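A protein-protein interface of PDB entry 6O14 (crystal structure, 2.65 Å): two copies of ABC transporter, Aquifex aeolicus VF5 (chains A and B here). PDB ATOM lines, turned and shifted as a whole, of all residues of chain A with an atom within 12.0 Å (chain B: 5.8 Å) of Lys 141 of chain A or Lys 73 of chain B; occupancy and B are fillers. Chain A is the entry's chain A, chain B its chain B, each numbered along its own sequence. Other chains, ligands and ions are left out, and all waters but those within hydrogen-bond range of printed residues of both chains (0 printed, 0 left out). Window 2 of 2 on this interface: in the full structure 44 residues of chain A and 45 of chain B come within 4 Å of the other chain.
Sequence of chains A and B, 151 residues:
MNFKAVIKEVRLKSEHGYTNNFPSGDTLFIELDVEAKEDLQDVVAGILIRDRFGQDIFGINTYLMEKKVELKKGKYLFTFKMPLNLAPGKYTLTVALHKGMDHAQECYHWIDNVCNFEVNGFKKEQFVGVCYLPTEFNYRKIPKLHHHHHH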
ATOM      1  N   PHE A 137     -10.786  23.068 -12.148  1.00  0.00           N
ATOM      2  CA  PHE A 137      -9.665  23.330 -13.037  1.00  0.00           C
ATOM      3  C   PHE A 137      -8.660  24.254 -12.366  1.00  0.00           C
ATOM      4  O   PHE A 137      -9.048  25.228 -11.718  1.00  0.00           O
ATOM      5  CB  PHE A 137     -10.158  23.955 -14.359  1.00  0.00           C
ATOM      6  CG  PHE A 137      -9.068  24.602 -15.170  1.00  0.00           C
ATOM      7  CD1 PHE A 137      -8.221  23.836 -15.944  1.00  0.00           C
ATOM      8  CD2 PHE A 137      -8.886  25.973 -15.145  1.00  0.00           C
ATOM      9  CE1 PHE A 137      -7.214  24.416 -16.676  1.00  0.00           C
ATOM     10  CE2 PHE A 137      -7.875  26.558 -15.880  1.00  0.00           C
ATOM     11  CZ  PHE A 137      -7.038  25.778 -16.644  1.00  0.00           C
ATOM     12  N   ASN A 138      -7.368  23.943 -12.519  1.00  0.00           N
ATOM     13  CA  ASN A 138      -6.309  24.812 -12.016  1.00  0.00           C
ATOM     14  C   ASN A 138      -5.112  24.751 -12.956  1.00  0.00           C
ATOM     15  O   ASN A 138      -4.929  23.785 -13.705  1.00  0.00           O
ATOM     16  CB  ASN A 138      -5.877  24.452 -10.589  1.00  0.00           C
ATOM     17  CG  ASN A 138      -5.233  25.635  -9.867  1.00  0.00           C
ATOM     18  OD1 ASN A 138      -5.809  26.726  -9.802  1.00  0.00           O
ATOM     19  ND2 ASN A 138      -4.023  25.431  -9.349  1.00  0.00           N
ATOM     20  N   TYR A 139      -4.297  25.803 -12.909  1.00  0.00           N
ATOM     21  CA  TYR A 139      -3.052  25.821 -13.661  1.00  0.00           C
ATOM     22  C   TYR A 139      -1.988  26.574 -12.878  1.00  0.00           C
ATOM     23  O   TYR A 139      -2.283  27.552 -12.185  1.00  0.00           O
ATOM     24  CB  TYR A 139      -3.240  26.429 -15.058  1.00  0.00           C
ATOM     25  CG  TYR A 139      -3.453  27.926 -15.107  1.00  0.00           C
ATOM     26  CD1 TYR A 139      -4.736  28.465 -15.102  1.00  0.00           C
ATOM     27  CD2 TYR A 139      -2.374  28.803 -15.211  1.00  0.00           C
ATOM     28  CE1 TYR A 139      -4.937  29.840 -15.168  1.00  0.00           C
ATOM     29  CE2 TYR A 139      -2.567  30.180 -15.276  1.00  0.00           C
ATOM     30  CZ  TYR A 139      -3.848  30.690 -15.255  1.00  0.00           C
ATOM     31  OH  TYR A 139      -4.053  32.047 -15.321  1.00  0.00           O
ATOM     32  N   ARG A 140      -0.753  26.090 -13.000  1.00  0.00           N
ATOM     33  CA  ARG A 140       0.407  26.581 -12.275  1.00  0.00           C
ATOM     34  C   ARG A 140       1.557  26.710 -13.266  1.00  0.00           C
ATOM     35  O   ARG A 140       1.746  25.838 -14.121  1.00  0.00           O
ATOM     36  CB  ARG A 140       0.831  25.627 -11.151  1.00  0.00           C
ATOM     37  CG  ARG A 140      -0.260  25.233 -10.183  1.00  0.00           C
ATOM     38  CD  ARG A 140       0.081  23.886  -9.589  1.00  0.00           C
ATOM     39  NE  ARG A 140       1.498  23.586  -9.770  1.00  0.00           N
ATOM     40  CZ  ARG A 140       2.010  22.363  -9.724  1.00  0.00           C
ATOM     41  NH1 ARG A 140       1.207  21.329  -9.503  1.00  0.00           N
ATOM     42  NH2 ARG A 140       3.316  22.174  -9.893  1.00  0.00           N
ATOM     43  N   LYS A 141       2.343  27.773 -13.151  1.00  0.00           N
ATOM     44  CA  LYS A 141       3.596  27.798 -13.885  1.00  0.00           C
ATOM     45  C   LYS A 141       4.571  26.866 -13.193  1.00  0.00           C
ATOM     46  O   LYS A 141       4.643  26.820 -11.962  1.00  0.00           O
ATOM     47  CB  LYS A 141       4.187  29.207 -13.965  1.00  0.00           C
ATOM     48  CG  LYS A 141       5.352  29.325 -14.954  1.00  0.00           C
ATOM     49  CD  LYS A 141       5.828  30.771 -15.132  1.00  0.00           C
ATOM     50  CE  LYS A 141       6.358  31.028 -16.549  1.00  0.00           C
ATOM     51  NZ  LYS A 141       5.462  31.955 -17.317  1.00  0.00           N
ATOM     52  N   ILE A 142       5.300  26.091 -13.979  1.00  0.00           N
ATOM     53  CA  ILE A 142       6.282  25.171 -13.417  1.00  0.00           C
ATOM     54  C   ILE A 142       7.654  25.635 -13.869  1.00  0.00           C
ATOM     55  O   ILE A 142       7.909  25.735 -15.079  1.00  0.00           O
ATOM     56  CB  ILE A 142       6.012  23.716 -13.833  1.00  0.00           C
ATOM     57  CG1 ILE A 142       5.648  23.627 -15.311  1.00  0.00           C
ATOM     58  CG2 ILE A 142       4.905  23.120 -12.962  1.00  0.00           C
ATOM     59  CD1 ILE A 142       5.205  22.241 -15.760  1.00  0.00           C
ATOM     60  N   PRO A 143       8.571  25.927 -12.952  1.00  0.00           N
ATOM     61  CA  PRO A 143       9.924  26.307 -13.349  1.00  0.00           C
ATOM     62  C   PRO A 143      10.703  25.084 -13.785  1.00  0.00           C
ATOM     63  O   PRO A 143      10.454  23.966 -13.327  1.00  0.00           O
ATOM     64  CB  PRO A 143      10.517  26.920 -12.073  1.00  0.00           C
ATOM     65  CG  PRO A 143       9.397  26.888 -11.033  1.00  0.00           C
ATOM     66  CD  PRO A 143       8.419  25.868 -11.490  1.00  0.00           C
ATOM     67  N   LYS A 144      11.681  25.311 -14.659  1.00  0.00           N
ATOM     68  CA  LYS A 144      12.450  24.201 -15.202  1.00  0.00           C
ATOM     69  C   LYS A 144      13.429  23.660 -14.158  1.00  0.00           C
ATOM     70  O   LYS A 144      14.335  22.887 -14.490  1.00  0.00           O
ATOM     71  CB  LYS A 144      13.156  24.617 -16.493  1.00  0.00           C
ATOM     72  CG  LYS A 144      13.999  25.879 -16.391  1.00  0.00           C
ATOM     73  CD  LYS A 144      15.450  25.547 -16.103  1.00  0.00           C
ATOM     74  CE  LYS A 144      16.331  26.766 -16.259  1.00  0.00           C
ATOM     75  NZ  LYS A 144      17.421  26.733 -15.267  1.00  0.00           N
ATOM     76  N   LEU A 145      13.263  24.066 -12.896  1.00  0.00           N
ATOM     77  CA  LEU A 145      13.846  23.337 -11.768  1.00  0.00           C
ATOM     78  C   LEU A 145      13.278  21.917 -11.687  1.00  0.00           C
ATOM     79  O   LEU A 145      12.090  21.687 -11.947  1.00  0.00           O
ATOM     80  CB  LEU A 145      13.586  24.063 -10.454  1.00  0.00           C
ATOM     81  CG  LEU A 145      14.753  24.594  -9.614  1.00  0.00           C
ATOM     82  CD1 LEU A 145      14.203  25.237  -8.339  1.00  0.00           C
ATOM     83  CD2 LEU A 145      15.778  23.498  -9.275  1.00  0.00           C
ATOM     84  N   ALA B  36       4.283  27.696 -23.430  1.00  0.00           N
ATOM     85  CA  ALA B  36       3.915  28.987 -24.000  1.00  0.00           C
ATOM     86  C   ALA B  36       5.180  29.610 -24.573  1.00  0.00           C
ATOM     87  O   ALA B  36       6.032  30.097 -23.827  1.00  0.00           O
ATOM     88  CB  ALA B  36       3.270  29.887 -22.948  1.00  0.00           C
ATOM     89  N   LYS B  37       5.295  29.591 -25.905  1.00  0.00           N
ATOM     90  CA  LYS B  37       6.449  30.175 -26.580  1.00  0.00           C
ATOM     91  C   LYS B  37       6.567  31.666 -26.326  1.00  0.00           C
ATOM     92  O   LYS B  37       7.630  32.247 -26.554  1.00  0.00           O
ATOM     93  CB  LYS B  37       6.364  29.915 -28.080  1.00  0.00           C
ATOM     94  CG  LYS B  37       5.919  28.508 -28.419  1.00  0.00           C
ATOM     95  CD  LYS B  37       6.869  27.488 -27.820  1.00  0.00           C
ATOM     96  CE  LYS B  37       6.550  26.080 -28.286  1.00  0.00           C
ATOM     97  NZ  LYS B  37       7.323  25.052 -27.528  1.00  0.00           N
ATOM     98  N   GLU B  38       5.503  32.288 -25.844  1.00  0.00           N
ATOM     99  CA  GLU B  38       5.425  33.733 -25.753  1.00  0.00           C
ATOM    100  C   GLU B  38       4.377  34.057 -24.697  1.00  0.00           C
ATOM    101  O   GLU B  38       3.895  33.164 -23.992  1.00  0.00           O
ATOM    102  CB  GLU B  38       5.096  34.300 -27.131  1.00  0.00           C
ATOM    103  CG  GLU B  38       5.280  35.758 -27.294  1.00  0.00           C
ATOM    104  CD  GLU B  38       4.750  36.187 -28.629  1.00  0.00           C
ATOM    105  OE1 GLU B  38       3.513  36.354 -28.716  1.00  0.00           O
ATOM    106  OE2 GLU B  38       5.553  36.322 -29.586  1.00  0.00           O
ATOM    107  N   ASP B  39       4.009  35.329 -24.587  1.00  0.00           N
ATOM    108  CA  ASP B  39       2.987  35.729 -23.634  1.00  0.00           C
ATOM    109  C   ASP B  39       1.617  35.667 -24.291  1.00  0.00           C
ATOM    110  O   ASP B  39       1.369  36.342 -25.295  1.00  0.00           O
ATOM    111  CB  ASP B  39       3.260  37.123 -23.089  1.00  0.00           C
ATOM    112  CG  ASP B  39       4.328  37.113 -22.032  1.00  0.00           C
ATOM    113  OD1 ASP B  39       4.846  36.010 -21.757  1.00  0.00           O
ATOM    114  OD2 ASP B  39       4.643  38.184 -21.471  1.00  0.00           O
ATOM    115  N   LEU B  71      -1.163  33.348 -19.614  1.00  0.00           N
ATOM    116  CA  LEU B  71       0.162  32.738 -19.505  1.00  0.00           C
ATOM    117  C   LEU B  71       1.270  33.729 -19.820  1.00  0.00           C
ATOM    118  O   LEU B  71       1.112  34.627 -20.647  1.00  0.00           O
ATOM    119  CB  LEU B  71       0.319  31.529 -20.435  1.00  0.00           C
ATOM    120  CG  LEU B  71      -0.888  30.619 -20.567  1.00  0.00           C
ATOM    121  CD1 LEU B  71      -0.651  29.582 -21.681  1.00  0.00           C
ATOM    122  CD2 LEU B  71      -1.230  29.978 -19.189  1.00  0.00           C
ATOM    123  N   LYS B  72       2.399  33.531 -19.165  1.00  0.00           N
ATOM    124  CA  LYS B  72       3.652  34.145 -19.547  1.00  0.00           C
ATOM    125  C   LYS B  72       4.583  33.041 -20.039  1.00  0.00           C
ATOM    126  O   LYS B  72       4.390  31.859 -19.732  1.00  0.00           O
ATOM    127  CB  LYS B  72       4.240  34.911 -18.365  1.00  0.00           C
ATOM    128  CG  LYS B  72       3.407  36.148 -17.999  1.00  0.00           C
ATOM    129  CD  LYS B  72       3.929  36.847 -16.755  1.00  0.00           C
ATOM    130  CE  LYS B  72       5.137  36.119 -16.204  1.00  0.00           C
ATOM    131  NZ  LYS B  72       5.769  36.801 -15.036  1.00  0.00           N
ATOM    132  N   LYS B  73       5.602  33.420 -20.809  1.00  0.00           N
ATOM    133  CA  LYS B  73       6.394  32.406 -21.495  1.00  0.00           C
ATOM    134  C   LYS B  73       7.087  31.496 -20.489  1.00  0.00           C
ATOM    135  O   LYS B  73       7.755  31.961 -19.559  1.00  0.00           O
ATOM    136  CB  LYS B  73       7.420  33.043 -22.433  1.00  0.00           C
ATOM    137  CG  LYS B  73       8.107  31.990 -23.324  1.00  0.00           C
ATOM    138  CD  LYS B  73       9.587  32.209 -23.584  1.00  0.00           C
ATOM    139  CE  LYS B  73       9.901  33.644 -23.954  1.00  0.00           C
ATOM    140  NZ  LYS B  73       9.263  33.995 -25.255  1.00  0.00           N
ATOM    141  N   GLY B  74       6.937  30.197 -20.700  1.00  0.00           N
ATOM    142  CA  GLY B  74       7.348  29.206 -19.732  1.00  0.00           C
ATOM    143  C   GLY B  74       6.470  27.973 -19.838  1.00  0.00           C
ATOM    144  O   GLY B  74       5.618  27.858 -20.716  1.00  0.00           O
ATOM    145  N   LYS B  75       6.692  27.053 -18.912  1.00  0.00           N
ATOM    146  CA  LYS B  75       5.961  25.801 -18.884  1.00  0.00           C
ATOM    147  C   LYS B  75       4.884  25.887 -17.819  1.00  0.00           C
ATOM    148  O   LYS B  75       5.031  26.581 -16.811  1.00  0.00           O
ATOM    149  CB  LYS B  75       6.888  24.626 -18.574  1.00  0.00           C
ATOM    150  CG  LYS B  75       7.772  24.182 -19.703  1.00  0.00           C
ATOM    151  CD  LYS B  75       8.324  22.802 -19.398  1.00  0.00           C
ATOM    152  CE  LYS B  75       7.201  21.824 -19.049  1.00  0.00           C
ATOM    153  NZ  LYS B  75       7.727  20.457 -18.763  1.00  0.00           N
ATOM    154  N   TYR B  76       3.778  25.206 -18.070  1.00  0.00           N
ATOM    155  CA  TYR B  76       2.647  25.228 -17.162  1.00  0.00           C
ATOM    156  C   TYR B  76       2.144  23.805 -16.961  1.00  0.00           C
ATOM    157  O   TYR B  76       2.489  22.887 -17.715  1.00  0.00           O
ATOM    158  CB  TYR B  76       1.516  26.122 -17.689  1.00  0.00           C
ATOM    159  CG  TYR B  76       1.774  27.609 -17.607  1.00  0.00           C
ATOM    160  CD1 TYR B  76       2.814  28.192 -18.310  1.00  0.00           C
ATOM    161  CD2 TYR B  76       0.947  28.435 -16.854  1.00  0.00           C
ATOM    162  CE1 TYR B  76       3.042  29.550 -18.251  1.00  0.00           C
ATOM    163  CE2 TYR B  76       1.164  29.795 -16.789  1.00  0.00           C
ATOM    164  CZ  TYR B  76       2.217  30.344 -17.490  1.00  0.00           C
ATOM    165  OH  TYR B  76       2.449  31.697 -17.435  1.00  0.00           O
ATOM    166  N   LEU B  77       1.331  23.625 -15.919  1.00  0.00           N
ATOM    167  CA  LEU B  77       0.577  22.393 -15.716  1.00  0.00           C
ATOM    168  C   LEU B  77      -0.903  22.747 -15.645  1.00  0.00           C
ATOM    169  O   LEU B  77      -1.308  23.561 -14.812  1.00  0.00           O
ATOM    170  CB  LEU B  77       1.038  21.661 -14.455  1.00  0.00           C
ATOM    171  CG  LEU B  77       0.326  20.344 -14.135  1.00  0.00           C
ATOM    172  CD1 LEU B  77       0.538  19.330 -15.243  1.00  0.00           C
ATOM    173  CD2 LEU B  77       0.810  19.793 -12.795  1.00  0.00           C
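The backbone NH (N) of Ile 142 of chain A sits at hydrogen-bond distance from the backbone carbonyl oxygen (O) of Lys 75 of chain B (2.9 Å).
NZ of Lys 141 of chain A is in hydrogen-bond range of OH of Tyr 76 of chain B.
N of Leu 77 of chain B lies within hydrogen-bond range of O of Arg 140 of chain A.
The backbone carbonyl oxygen (O) of Lys 73 of chain B is in hydrogen-bond range of the side-chain amino group (NZ) of Lys 141 of chain A (3.2 Å).
NZ of Lys 141 of chain A lies within hydrogen-bond range of O of Lys 72 of chain B (2.6 Å).
Printed residues of chain A that touch a printed residue of chain B: Asn 138, Tyr 139, Arg 140, Lys 141 and Ile 142.
Of the 11 printed residues of chain B, 6 touch a printed residue of chain A.
Among the printed residues, no Asp or Glu carboxylate lies within 4 Å of a Lys or Arg side-chain nitrogen of the other chain.
Lys 141 of chain A touches just these residues of chain B: Lys 72, Lys 73, Gly 74, Lys 75 and Tyr 76.
Lys 73 of chain B touches just one residue of chain A: Lys 141 (3.2 Å).
No residue of chain A comes within 4 Å of Ala 36 of chain B.
No residue of chain A comes within 4 Å of Glu 38 of chain B.
Asp 39 of chain B touches none of the printed residues of chain A.
No residue of chain A comes within 4 Å of Leu 71 of chain B.
Lys 72 of chain B touches one residue of chain A.
Of the printed residues of chain A, Gly 74 of chain B touches Lys 141.
Of chain A, only Tyr 139, Arg 140, Lys 141 and Ile 142 come within 4 Å of Tyr 76 of chain B.
Of the printed residues of chain B, Tyr 139 of chain A touches Tyr 76 and Leu 77.
Of the printed residues of chain B, Arg 140 of chain A touches Tyr 76 and Leu 77.
Of the printed residues of chain B, Ile 142 of chain A touches Lys 75 and Tyr 76.
Of the printed residues of chain A, Lys 75 of chain B touches Lys 141 and Ile 142.
Lys 144 of chain A touches none of the printed residues of chain B.
The nearest residue of chain A that does not touch Lys 73 of chain B is Ile 142 of chain A (7.7 Å).
The nearest printed residue of chain B that does not touch Arg 140 of chain A is Lys 75 of chain B (4.3 Å).
Among the printed residues, merely in contact across the chains: Asn 138 of chain A with Leu 77 of chain B (3.8 Å), Tyr 139 of chain A with Tyr 76 of chain B (3.7 Å), Tyr 139 of chain A with Leu 77 of chain B (3.1 Å), Arg 140 of chain A with Tyr 76 of chain B (3.2 Å), Lys 141 of chain A with Gly 74 of chain B (3.8 Å), Lys 141 of chain A with Lys 75 of chain B (3.3 Å) and Ile 142 of chain A with Tyr 76 of chain B (3.4 Å).
N of Ala 36 of chain B lies within hydrogen-bond range of O of Gly 74 of chain B (3.0 Å).
The backbone carbonyl oxygen (O) of Lys 37 of chain B is in hydrogen-bond range of the side-chain amino group (NZ) of Lys 73 of chain B, at 2.7 Å.
The backbone NH of Lys 72 of chain B lies within hydrogen-bond range of the side-chain hydroxyl of Tyr 76 of chain B, at 2.5 Å.
OD1 of Asp 39 of chain B sits at hydrogen-bond distance from N of Lys 73 of chain B (2.9 Å).
No position is printed for both chains.
Of the 12 pairs that touch across the chains among the printed residues, none has its exchanged pair printed and touching as well.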
